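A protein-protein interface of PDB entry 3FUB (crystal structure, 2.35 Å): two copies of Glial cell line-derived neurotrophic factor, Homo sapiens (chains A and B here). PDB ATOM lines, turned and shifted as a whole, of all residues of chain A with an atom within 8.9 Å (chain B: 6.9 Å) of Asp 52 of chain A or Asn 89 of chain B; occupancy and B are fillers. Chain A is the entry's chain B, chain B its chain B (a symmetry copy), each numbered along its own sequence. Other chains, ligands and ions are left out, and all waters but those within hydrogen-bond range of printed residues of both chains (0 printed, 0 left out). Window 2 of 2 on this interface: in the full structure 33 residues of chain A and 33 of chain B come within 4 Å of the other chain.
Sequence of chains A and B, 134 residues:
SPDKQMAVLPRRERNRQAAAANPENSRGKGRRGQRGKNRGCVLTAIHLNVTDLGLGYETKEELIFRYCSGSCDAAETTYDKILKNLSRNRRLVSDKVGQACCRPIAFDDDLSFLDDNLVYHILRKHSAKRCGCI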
ATOM      1  N   ILE A  46      -9.408  12.641  27.940  1.00  0.00           N
ATOM      2  CA  ILE A  46      -8.039  12.280  28.328  1.00  0.00           C
ATOM      3  C   ILE A  46      -7.383  13.316  29.259  1.00  0.00           C
ATOM      4  O   ILE A  46      -7.556  14.526  29.089  1.00  0.00           O
ATOM      5  CB  ILE A  46      -7.135  11.961  27.089  1.00  0.00           C
ATOM      6  CG1 ILE A  46      -5.779  11.394  27.534  1.00  0.00           C
ATOM      7  CG2 ILE A  46      -6.979  13.182  26.181  1.00  0.00           C
ATOM      8  CD1 ILE A  46      -5.047  10.588  26.478  1.00  0.00           C
ATOM      9  N   HIS A  47      -6.647  12.812  30.249  1.00  0.00           N
ATOM     10  CA  HIS A  47      -5.911  13.630  31.212  1.00  0.00           C
ATOM     11  C   HIS A  47      -4.499  13.949  30.694  1.00  0.00           C
ATOM     12  O   HIS A  47      -3.660  13.053  30.564  1.00  0.00           O
ATOM     13  CB  HIS A  47      -5.863  12.902  32.564  1.00  0.00           C
ATOM     14  CG  HIS A  47      -5.151  13.654  33.649  1.00  0.00           C
ATOM     15  ND1 HIS A  47      -4.377  13.024  34.600  1.00  0.00           N
ATOM     16  CD2 HIS A  47      -5.096  14.977  33.935  1.00  0.00           C
ATOM     17  CE1 HIS A  47      -3.879  13.926  35.429  1.00  0.00           C
ATOM     18  NE2 HIS A  47      -4.297  15.119  35.045  1.00  0.00           N
ATOM     19  N   LEU A  48      -4.245  15.226  30.403  1.00  0.00           N
ATOM     20  CA  LEU A  48      -2.980  15.648  29.780  1.00  0.00           C
ATOM     21  C   LEU A  48      -2.250  16.770  30.514  1.00  0.00           C
ATOM     22  O   LEU A  48      -2.836  17.486  31.324  1.00  0.00           O
ATOM     23  CB  LEU A  48      -3.225  16.111  28.339  1.00  0.00           C
ATOM     24  CG  LEU A  48      -3.882  15.193  27.305  1.00  0.00           C
ATOM     25  CD1 LEU A  48      -4.419  16.038  26.163  1.00  0.00           C
ATOM     26  CD2 LEU A  48      -2.911  14.134  26.790  1.00  0.00           C
ATOM     27  N   ASN A  49      -0.964  16.912  30.206  1.00  0.00           N
ATOM     28  CA  ASN A  49      -0.206  18.110  30.539  1.00  0.00           C
ATOM     29  C   ASN A  49      -0.557  19.233  29.564  1.00  0.00           C
ATOM     30  O   ASN A  49      -0.849  18.969  28.400  1.00  0.00           O
ATOM     31  CB  ASN A  49       1.292  17.823  30.455  1.00  0.00           C
ATOM     32  CG  ASN A  49       1.845  17.179  31.716  1.00  0.00           C
ATOM     33  OD1 ASN A  49       1.754  17.743  32.806  1.00  0.00           O
ATOM     34  ND2 ASN A  49       2.436  15.996  31.567  1.00  0.00           N
ATOM     35  N   VAL A  50      -0.518  20.479  30.027  1.00  0.00           N
ATOM     36  CA  VAL A  50      -0.781  21.634  29.156  1.00  0.00           C
ATOM     37  C   VAL A  50       0.256  21.743  28.030  1.00  0.00           C
ATOM     38  O   VAL A  50      -0.037  22.257  26.943  1.00  0.00           O
ATOM     39  CB  VAL A  50      -0.841  22.960  29.953  1.00  0.00           C
ATOM     40  CG1 VAL A  50      -0.861  24.164  29.010  1.00  0.00           C
ATOM     41  CG2 VAL A  50      -2.066  22.983  30.856  1.00  0.00           C
ATOM     42  N   THR A  51       1.462  21.253  28.300  1.00  0.00           N
ATOM     43  CA  THR A  51       2.534  21.227  27.309  1.00  0.00           C
ATOM     44  C   THR A  51       2.277  20.204  26.206  1.00  0.00           C
ATOM     45  O   THR A  51       2.784  20.359  25.096  1.00  0.00           O
ATOM     46  CB  THR A  51       3.904  20.948  27.954  1.00  0.00           C
ATOM     47  OG1 THR A  51       3.818  19.787  28.789  1.00  0.00           O
ATOM     48  CG2 THR A  51       4.359  22.143  28.779  1.00  0.00           C
ATOM     49  N   ASP A  52       1.492  19.168  26.518  1.00  0.00           N
ATOM     50  CA  ASP A  52       1.082  18.147  25.538  1.00  0.00           C
ATOM     51  C   ASP A  52       0.232  18.745  24.410  1.00  0.00           C
ATOM     52  O   ASP A  52       0.126  18.163  23.328  1.00  0.00           O
ATOM     53  CB  ASP A  52       0.297  17.008  26.219  1.00  0.00           C
ATOM     54  CG  ASP A  52       1.127  16.232  27.245  1.00  0.00           C
ATOM     55  OD1 ASP A  52       2.370  16.178  27.115  1.00  0.00           O
ATOM     56  OD2 ASP A  52       0.526  15.661  28.186  1.00  0.00           O
ATOM     57  N   LEU A  53      -0.366  19.908  24.674  1.00  0.00           N
ATOM     58  CA  LEU A  53      -1.245  20.587  23.719  1.00  0.00           C
ATOM     59  C   LEU A  53      -0.462  21.358  22.665  1.00  0.00           C
ATOM     60  O   LEU A  53      -0.994  21.677  21.599  1.00  0.00           O
ATOM     61  CB  LEU A  53      -2.179  21.559  24.445  1.00  0.00           C
ATOM     62  CG  LEU A  53      -2.892  21.125  25.723  1.00  0.00           C
ATOM     63  CD1 LEU A  53      -3.641  22.320  26.273  1.00  0.00           C
ATOM     64  CD2 LEU A  53      -3.831  19.949  25.498  1.00  0.00           C
ATOM     65  N   GLY A  54       0.789  21.674  22.989  1.00  0.00           N
ATOM     66  CA  GLY A  54       1.690  22.369  22.086  1.00  0.00           C
ATOM     67  C   GLY A  54       1.197  23.723  21.618  1.00  0.00           C
ATOM     68  O   GLY A  54       1.272  24.027  20.424  1.00  0.00           O
ATOM     69  N   LEU A  55       0.705  24.540  22.551  1.00  0.00           N
ATOM     70  CA  LEU A  55       0.171  25.867  22.216  1.00  0.00           C
ATOM     71  C   LEU A  55       1.130  27.032  22.531  1.00  0.00           C
ATOM     72  O   LEU A  55       0.736  28.203  22.516  1.00  0.00           O
ATOM     73  CB  LEU A  55      -1.211  26.078  22.858  1.00  0.00           C
ATOM     74  CG  LEU A  55      -2.379  25.211  22.353  1.00  0.00           C
ATOM     75  CD1 LEU A  55      -3.546  25.217  23.346  1.00  0.00           C
ATOM     76  CD2 LEU A  55      -2.856  25.635  20.962  1.00  0.00           C
ATOM     77  N   GLY A  56       2.387  26.701  22.800  1.00  0.00           N
ATOM     78  CA  GLY A  56       3.425  27.714  23.008  1.00  0.00           C
ATOM     79  C   GLY A  56       3.811  27.939  24.455  1.00  0.00           C
ATOM     80  O   GLY A  56       4.592  28.839  24.757  1.00  0.00           O
ATOM     81  N   TYR A  57       3.285  27.112  25.353  1.00  0.00           N
ATOM     82  CA  TYR A  57       3.438  27.368  26.779  1.00  0.00           C
ATOM     83  C   TYR A  57       4.505  26.509  27.430  1.00  0.00           C
ATOM     84  O   TYR A  57       4.706  25.364  27.049  1.00  0.00           O
ATOM     85  CB  TYR A  57       2.101  27.200  27.516  1.00  0.00           C
ATOM     86  CG  TYR A  57       0.957  27.993  26.922  1.00  0.00           C
ATOM     87  CD1 TYR A  57       0.907  29.382  27.038  1.00  0.00           C
ATOM     88  CD2 TYR A  57      -0.078  27.348  26.248  1.00  0.00           C
ATOM     89  CE1 TYR A  57      -0.147  30.110  26.498  1.00  0.00           C
ATOM     90  CE2 TYR A  57      -1.128  28.063  25.707  1.00  0.00           C
ATOM     91  CZ  TYR A  57      -1.163  29.440  25.837  1.00  0.00           C
ATOM     92  OH  TYR A  57      -2.212  30.141  25.292  1.00  0.00           O
ATOM     93  N   THR A  59       4.954  25.279  30.987  1.00  0.00           N
ATOM     94  CA  THR A  59       4.329  25.138  32.295  1.00  0.00           C
ATOM     95  C   THR A  59       4.334  23.689  32.769  1.00  0.00           C
ATOM     96  O   THR A  59       4.702  22.783  32.022  1.00  0.00           O
ATOM     97  CB  THR A  59       2.874  25.684  32.287  1.00  0.00           C
ATOM     98  OG1 THR A  59       2.345  25.676  33.620  1.00  0.00           O
ATOM     99  CG2 THR A  59       1.974  24.856  31.367  1.00  0.00           C
ATOM    100  N   LYS A  60       3.930  23.490  34.019  1.00  0.00           N
ATOM    101  CA  LYS A  60       3.793  22.158  34.599  1.00  0.00           C
ATOM    102  C   LYS A  60       2.328  21.888  34.921  1.00  0.00           C
ATOM    103  O   LYS A  60       1.989  20.828  35.447  1.00  0.00           O
ATOM    104  CB  LYS A  60       4.627  22.042  35.877  1.00  0.00           C
ATOM    105  CG  LYS A  60       6.119  22.299  35.711  1.00  0.00           C
ATOM    106  CD  LYS A  60       6.850  21.062  35.220  1.00  0.00           C
ATOM    107  CE  LYS A  60       8.332  21.354  35.005  1.00  0.00           C
ATOM    108  NZ  LYS A  60       8.573  22.303  33.871  1.00  0.00           N
ATOM    109  N   GLU A  61       1.470  22.856  34.608  1.00  0.00           N
ATOM    110  CA  GLU A  61       0.048  22.760  34.923  1.00  0.00           C
ATOM    111  C   GLU A  61      -0.659  21.770  33.993  1.00  0.00           C
ATOM    112  O   GLU A  61      -0.112  21.388  32.957  1.00  0.00           O
ATOM    113  CB  GLU A  61      -0.624  24.142  34.913  1.00  0.00           C
ATOM    114  CG  GLU A  61      -0.250  25.026  36.113  1.00  0.00           C
ATOM    115  CD  GLU A  61      -1.445  25.745  36.754  1.00  0.00           C
ATOM    116  OE1 GLU A  61      -2.547  25.154  36.840  1.00  0.00           O
ATOM    117  OE2 GLU A  61      -1.273  26.904  37.194  1.00  0.00           O
ATOM    118  N   GLU A  62      -1.860  21.345  34.378  1.00  0.00           N
ATOM    119  CA  GLU A  62      -2.517  20.201  33.742  1.00  0.00           C
ATOM    120  C   GLU A  62      -3.987  20.452  33.399  1.00  0.00           C
ATOM    121  O   GLU A  62      -4.562  21.465  33.804  1.00  0.00           O
ATOM    122  CB  GLU A  62      -2.402  18.968  34.646  1.00  0.00           C
ATOM    123  CG  GLU A  62      -0.978  18.580  35.018  1.00  0.00           C
ATOM    124  CD  GLU A  62      -0.870  17.168  35.575  1.00  0.00           C
ATOM    125  OE1 GLU A  62      -1.915  16.488  35.730  1.00  0.00           O
ATOM    126  OE2 GLU A  62       0.271  16.735  35.851  1.00  0.00           O
ATOM    127  N   LEU A  63      -4.587  19.523  32.653  1.00  0.00           N
ATOM    128  CA  LEU A  63      -5.999  19.627  32.272  1.00  0.00           C
ATOM    129  C   LEU A  63      -6.676  18.289  31.935  1.00  0.00           C
ATOM    130  O   LEU A  63      -6.025  17.251  31.815  1.00  0.00           O
ATOM    131  CB  LEU A  63      -6.182  20.636  31.122  1.00  0.00           C
ATOM    132  CG  LEU A  63      -5.837  20.336  29.654  1.00  0.00           C
ATOM    133  CD1 LEU A  63      -6.318  21.478  28.779  1.00  0.00           C
ATOM    134  CD2 LEU A  63      -4.351  20.100  29.424  1.00  0.00           C
ATOM    135  N   PHE A  65      -8.642  17.143  28.737  1.00  0.00           N
ATOM    136  CA  PHE A  65      -9.018  17.525  27.381  1.00  0.00           C
ATOM    137  C   PHE A  65     -10.078  16.562  26.848  1.00  0.00           C
ATOM    138  O   PHE A  65      -9.941  15.343  26.976  1.00  0.00           O
ATOM    139  CB  PHE A  65      -7.784  17.583  26.476  1.00  0.00           C
ATOM    140  CG  PHE A  65      -8.105  17.761  25.018  1.00  0.00           C
ATOM    141  CD1 PHE A  65      -8.514  18.997  24.522  1.00  0.00           C
ATOM    142  CD2 PHE A  65      -8.002  16.686  24.138  1.00  0.00           C
ATOM    143  CE1 PHE A  65      -8.821  19.156  23.172  1.00  0.00           C
ATOM    144  CE2 PHE A  65      -8.301  16.837  22.788  1.00  0.00           C
ATOM    145  CZ  PHE A  65      -8.712  18.075  22.302  1.00  0.00           C
ATOM    146  N   ILE B  82      -5.084  21.740  18.946  1.00  0.00           N
ATOM    147  CA  ILE B  82      -4.818  20.676  19.910  1.00  0.00           C
ATOM    148  C   ILE B  82      -4.963  19.288  19.285  1.00  0.00           C
ATOM    149  O   ILE B  82      -4.177  18.388  19.594  1.00  0.00           O
ATOM    150  CB  ILE B  82      -5.685  20.815  21.188  1.00  0.00           C
ATOM    151  CG1 ILE B  82      -5.390  22.150  21.883  1.00  0.00           C
ATOM    152  CG2 ILE B  82      -5.428  19.642  22.140  1.00  0.00           C
ATOM    153  CD1 ILE B  82      -6.273  22.454  23.081  1.00  0.00           C
ATOM    154  N   LYS B  84      -4.521  18.469  16.043  1.00  0.00           N
ATOM    155  CA  LYS B  84      -3.353  18.329  15.174  1.00  0.00           C
ATOM    156  C   LYS B  84      -2.069  18.064  15.975  1.00  0.00           C
ATOM    157  O   LYS B  84      -1.259  17.214  15.597  1.00  0.00           O
ATOM    158  CB  LYS B  84      -3.223  19.557  14.251  1.00  0.00           C
ATOM    159  CG  LYS B  84      -1.813  19.867  13.742  1.00  0.00           C
ATOM    160  CD  LYS B  84      -1.791  21.029  12.754  1.00  0.00           C
ATOM    161  CE  LYS B  84      -1.802  20.529  11.310  1.00  0.00           C
ATOM    162  NZ  LYS B  84      -1.566  21.619  10.313  1.00  0.00           N
ATOM    163  N   ASN B  85      -1.895  18.778  17.085  1.00  0.00           N
ATOM    164  CA  ASN B  85      -0.718  18.578  17.935  1.00  0.00           C
ATOM    165  C   ASN B  85      -0.705  17.234  18.657  1.00  0.00           C
ATOM    166  O   ASN B  85       0.342  16.587  18.737  1.00  0.00           O
ATOM    167  CB  ASN B  85      -0.533  19.734  18.925  1.00  0.00           C
ATOM    168  CG  ASN B  85      -0.142  21.040  18.238  1.00  0.00           C
ATOM    169  OD1 ASN B  85       0.095  21.082  17.027  1.00  0.00           O
ATOM    170  ND2 ASN B  85      -0.084  22.114  19.013  1.00  0.00           N
ATOM    171  N   LEU B  86      -1.863  16.819  19.173  1.00  0.00           N
ATOM    172  CA  LEU B  86      -1.996  15.514  19.830  1.00  0.00           C
ATOM    173  C   LEU B  86      -1.791  14.347  18.868  1.00  0.00           C
ATOM    174  O   LEU B  86      -1.338  13.275  19.275  1.00  0.00           O
ATOM    175  CB  LEU B  86      -3.349  15.368  20.537  1.00  0.00           C
ATOM    176  CG  LEU B  86      -3.558  16.030  21.906  1.00  0.00           C
ATOM    177  CD1 LEU B  86      -4.849  15.511  22.525  1.00  0.00           C
ATOM    178  CD2 LEU B  86      -2.380  15.809  22.861  1.00  0.00           C
ATOM    179  N   SER B  87      -2.139  14.560  17.600  1.00  0.00           N
ATOM    180  CA  SER B  87      -1.948  13.553  16.562  1.00  0.00           C
ATOM    181  C   SER B  87      -0.457  13.349  16.267  1.00  0.00           C
ATOM    182  O   SER B  87       0.015  12.215  16.199  1.00  0.00           O
ATOM    183  CB  SER B  87      -2.702  13.947  15.286  1.00  0.00           C
ATOM    184  OG  SER B  87      -2.679  12.897  14.334  1.00  0.00           O
ATOM    185  N   ARG B  88       0.267  14.456  16.108  1.00  0.00           N
ATOM    186  CA  ARG B  88       1.705  14.437  15.834  1.00  0.00           C
ATOM    187  C   ARG B  88       2.518  13.744  16.935  1.00  0.00           C
ATOM    188  O   ARG B  88       3.306  12.841  16.644  1.00  0.00           O
ATOM    189  CB  ARG B  88       2.214  15.857  15.591  1.00  0.00           C
ATOM    190  CG  ARG B  88       3.686  15.948  15.274  1.00  0.00           C
ATOM    191  CD  ARG B  88       4.042  17.349  14.854  1.00  0.00           C
ATOM    192  NE  ARG B  88       5.485  17.514  14.750  1.00  0.00           N
ATOM    193  CZ  ARG B  88       6.238  18.071  15.689  1.00  0.00           C
ATOM    194  NH1 ARG B  88       5.687  18.523  16.803  1.00  0.00           N
ATOM    195  NH2 ARG B  88       7.541  18.175  15.517  1.00  0.00           N
ATOM    196  N   ASN B  89       2.324  14.149  18.190  1.00  0.00           N
ATOM    197  CA  ASN B  89       2.980  13.456  19.307  1.00  0.00           C
ATOM    198  C   ASN B  89       2.309  12.127  19.680  1.00  0.00           C
ATOM    199  O   ASN B  89       2.720  11.466  20.632  1.00  0.00           O
ATOM    200  CB  ASN B  89       3.195  14.373  20.531  1.00  0.00           C
ATOM    201  CG  ASN B  89       1.907  15.004  21.048  1.00  0.00           C
ATOM    202  OD1 ASN B  89       0.831  14.415  20.974  1.00  0.00           O
ATOM    203  ND2 ASN B  89       2.024  16.211  21.595  1.00  0.00           N
ATOM    204  N   ARG B  90       1.282  11.750  18.913  1.00  0.00           N
ATOM    205  CA  ARG B  90       0.605  10.444  19.014  1.00  0.00           C
ATOM    206  C   ARG B  90       0.059  10.092  20.406  1.00  0.00           C
ATOM    207  O   ARG B  90       0.023   8.918  20.797  1.00  0.00           O
ATOM    208  CB  ARG B  90       1.508   9.319  18.484  1.00  0.00           C
ATOM    209  N   ARG B  91      -0.364  11.119  21.140  1.00  0.00           N
ATOM    210  CA  ARG B  91      -1.039  10.940  22.423  1.00  0.00           C
ATOM    211  C   ARG B  91      -2.554  11.075  22.251  1.00  0.00           C
ATOM    212  O   ARG B  91      -3.265  11.430  23.195  1.00  0.00           O
ATOM    213  CB  ARG B  91      -0.524  11.955  23.455  1.00  0.00           C
ATOM    214  N   LEU B  92      -3.044  10.791  21.045  1.00  0.00           N
ATOM    215  CA  LEU B  92      -4.466  10.924  20.762  1.00  0.00           C
ATOM    216  C   LEU B  92      -5.132   9.557  20.738  1.00  0.00           C
ATOM    217  O   LEU B  92      -5.454   9.001  21.789  1.00  0.00           O
ATOM    218  CB  LEU B  92      -4.703  11.678  19.447  1.00  0.00           C
ATOM    219  CG  LEU B  92      -5.895  12.654  19.408  1.00  0.00           C
ATOM    220  CD1 LEU B  92      -5.810  13.586  18.205  1.00  0.00           C
ATOM    221  CD2 LEU B  92      -7.257  11.958  19.437  1.00  0.00           C
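The side-chain amide nitrogen (ND2) of Asn 89 of chain B lies within hydrogen-bond range of the backbone carbonyl oxygen (O) of Asp 52 of chain A, at 3.2 Å.
The backbone carbonyl oxygen of Leu 53 of chain A is in hydrogen-bond range of the side-chain amide nitrogen of Asn 85 of chain B (2.8 Å).
The backbone carbonyl oxygen (O) of Gly 54 of chain A sits at hydrogen-bond distance from the side-chain amide nitrogen (ND2) of Asn 85 of chain B.
The backbone carbonyl oxygen (O) of Leu 48 of chain A is in hydrogen-bond range of the backbone NH (N) of Leu 63 of chain A (3.0 Å).
The side-chain carboxylate of Asp 52 of chain A is in hydrogen-bond range of the backbone NH of Asn 49 of chain A.
The side-chain amide oxygen (OD1) of Asn 89 of chain B sits close to the backbone carbonyl oxygen (O) of Asn 85 of chain B (3.2 Å).
The side-chain amide oxygen (OD1) of Asn 89 of chain B sits close to the backbone carbonyl oxygen (O) of Leu 86 of chain B (3.0 Å).
The backbone carbonyl oxygen (O) of Leu 86 of chain B sits at hydrogen-bond distance from the backbone NH (N) of Arg 91 of chain B.
N of Leu 92 of chain B is in hydrogen-bond range of O of Leu 86 of chain B (3.5 Å).
Arg 91 of chain B touches Ile 46 of chain A.
Leu 48 of chain A touches Leu 86 of chain B (CD1 to CD1, 3.7 Å).
Asp 52 of chain A touches Leu 86 of chain B.
Leu 53 of chain A touches Ile 82 of chain B (CD2 to CG2, 3.7 Å).
Leu 55 of chain A touches Ile 82 of chain B (CD1 to CG1, 3.9 Å).
Phe 65 of chain A touches Ile 82 of chain B.
CD1 of Leu 86 of chain B touches CE2 of Phe 65 of chain A, at 3.7 Å.
Asp 52 of chain A touches just these residues of chain B: Leu 86 (3.5 Å) and Asn 89 (3.2 Å).
Of the printed residues of chain A, Asn 89 of chain B touches Asp 52 (3.2 Å).
Of the printed residues of chain A, Leu 86 of chain B touches Leu 48, Asp 52 and Phe 65.
Of the printed residues of chain B, Gly 54 of chain A touches Asn 85 (2.7 Å).
Thr 59 of chain A touches none of the printed residues of chain B.
The nearest residue of chain B that does not touch Asp 52 of chain A is Asn 85 of chain B (4.7 Å).
The nearest residue of chain A that does not touch Asn 89 of chain B is Leu 53 of chain A (5.4 Å).
The nearest printed residue of chain B that does not touch Leu 48 of chain A is Arg 91 of chain B (4.5 Å).
Of the 10 printed residues of chain B, 5 touch a printed residue of chain A.
Hydrophobic or aromatic side chains of chain B that line the printed part of chain A: Ile 82 and Leu 86.
Of the 18 printed residues of chain A, 7 touch a printed residue of chain B.
Printed residues of chain A that touch a printed residue of chain B: Ile 46, Leu 48, Asp 52, Leu 53, Gly 54, Leu 55 and Phe 65.
No position is printed for both chains.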
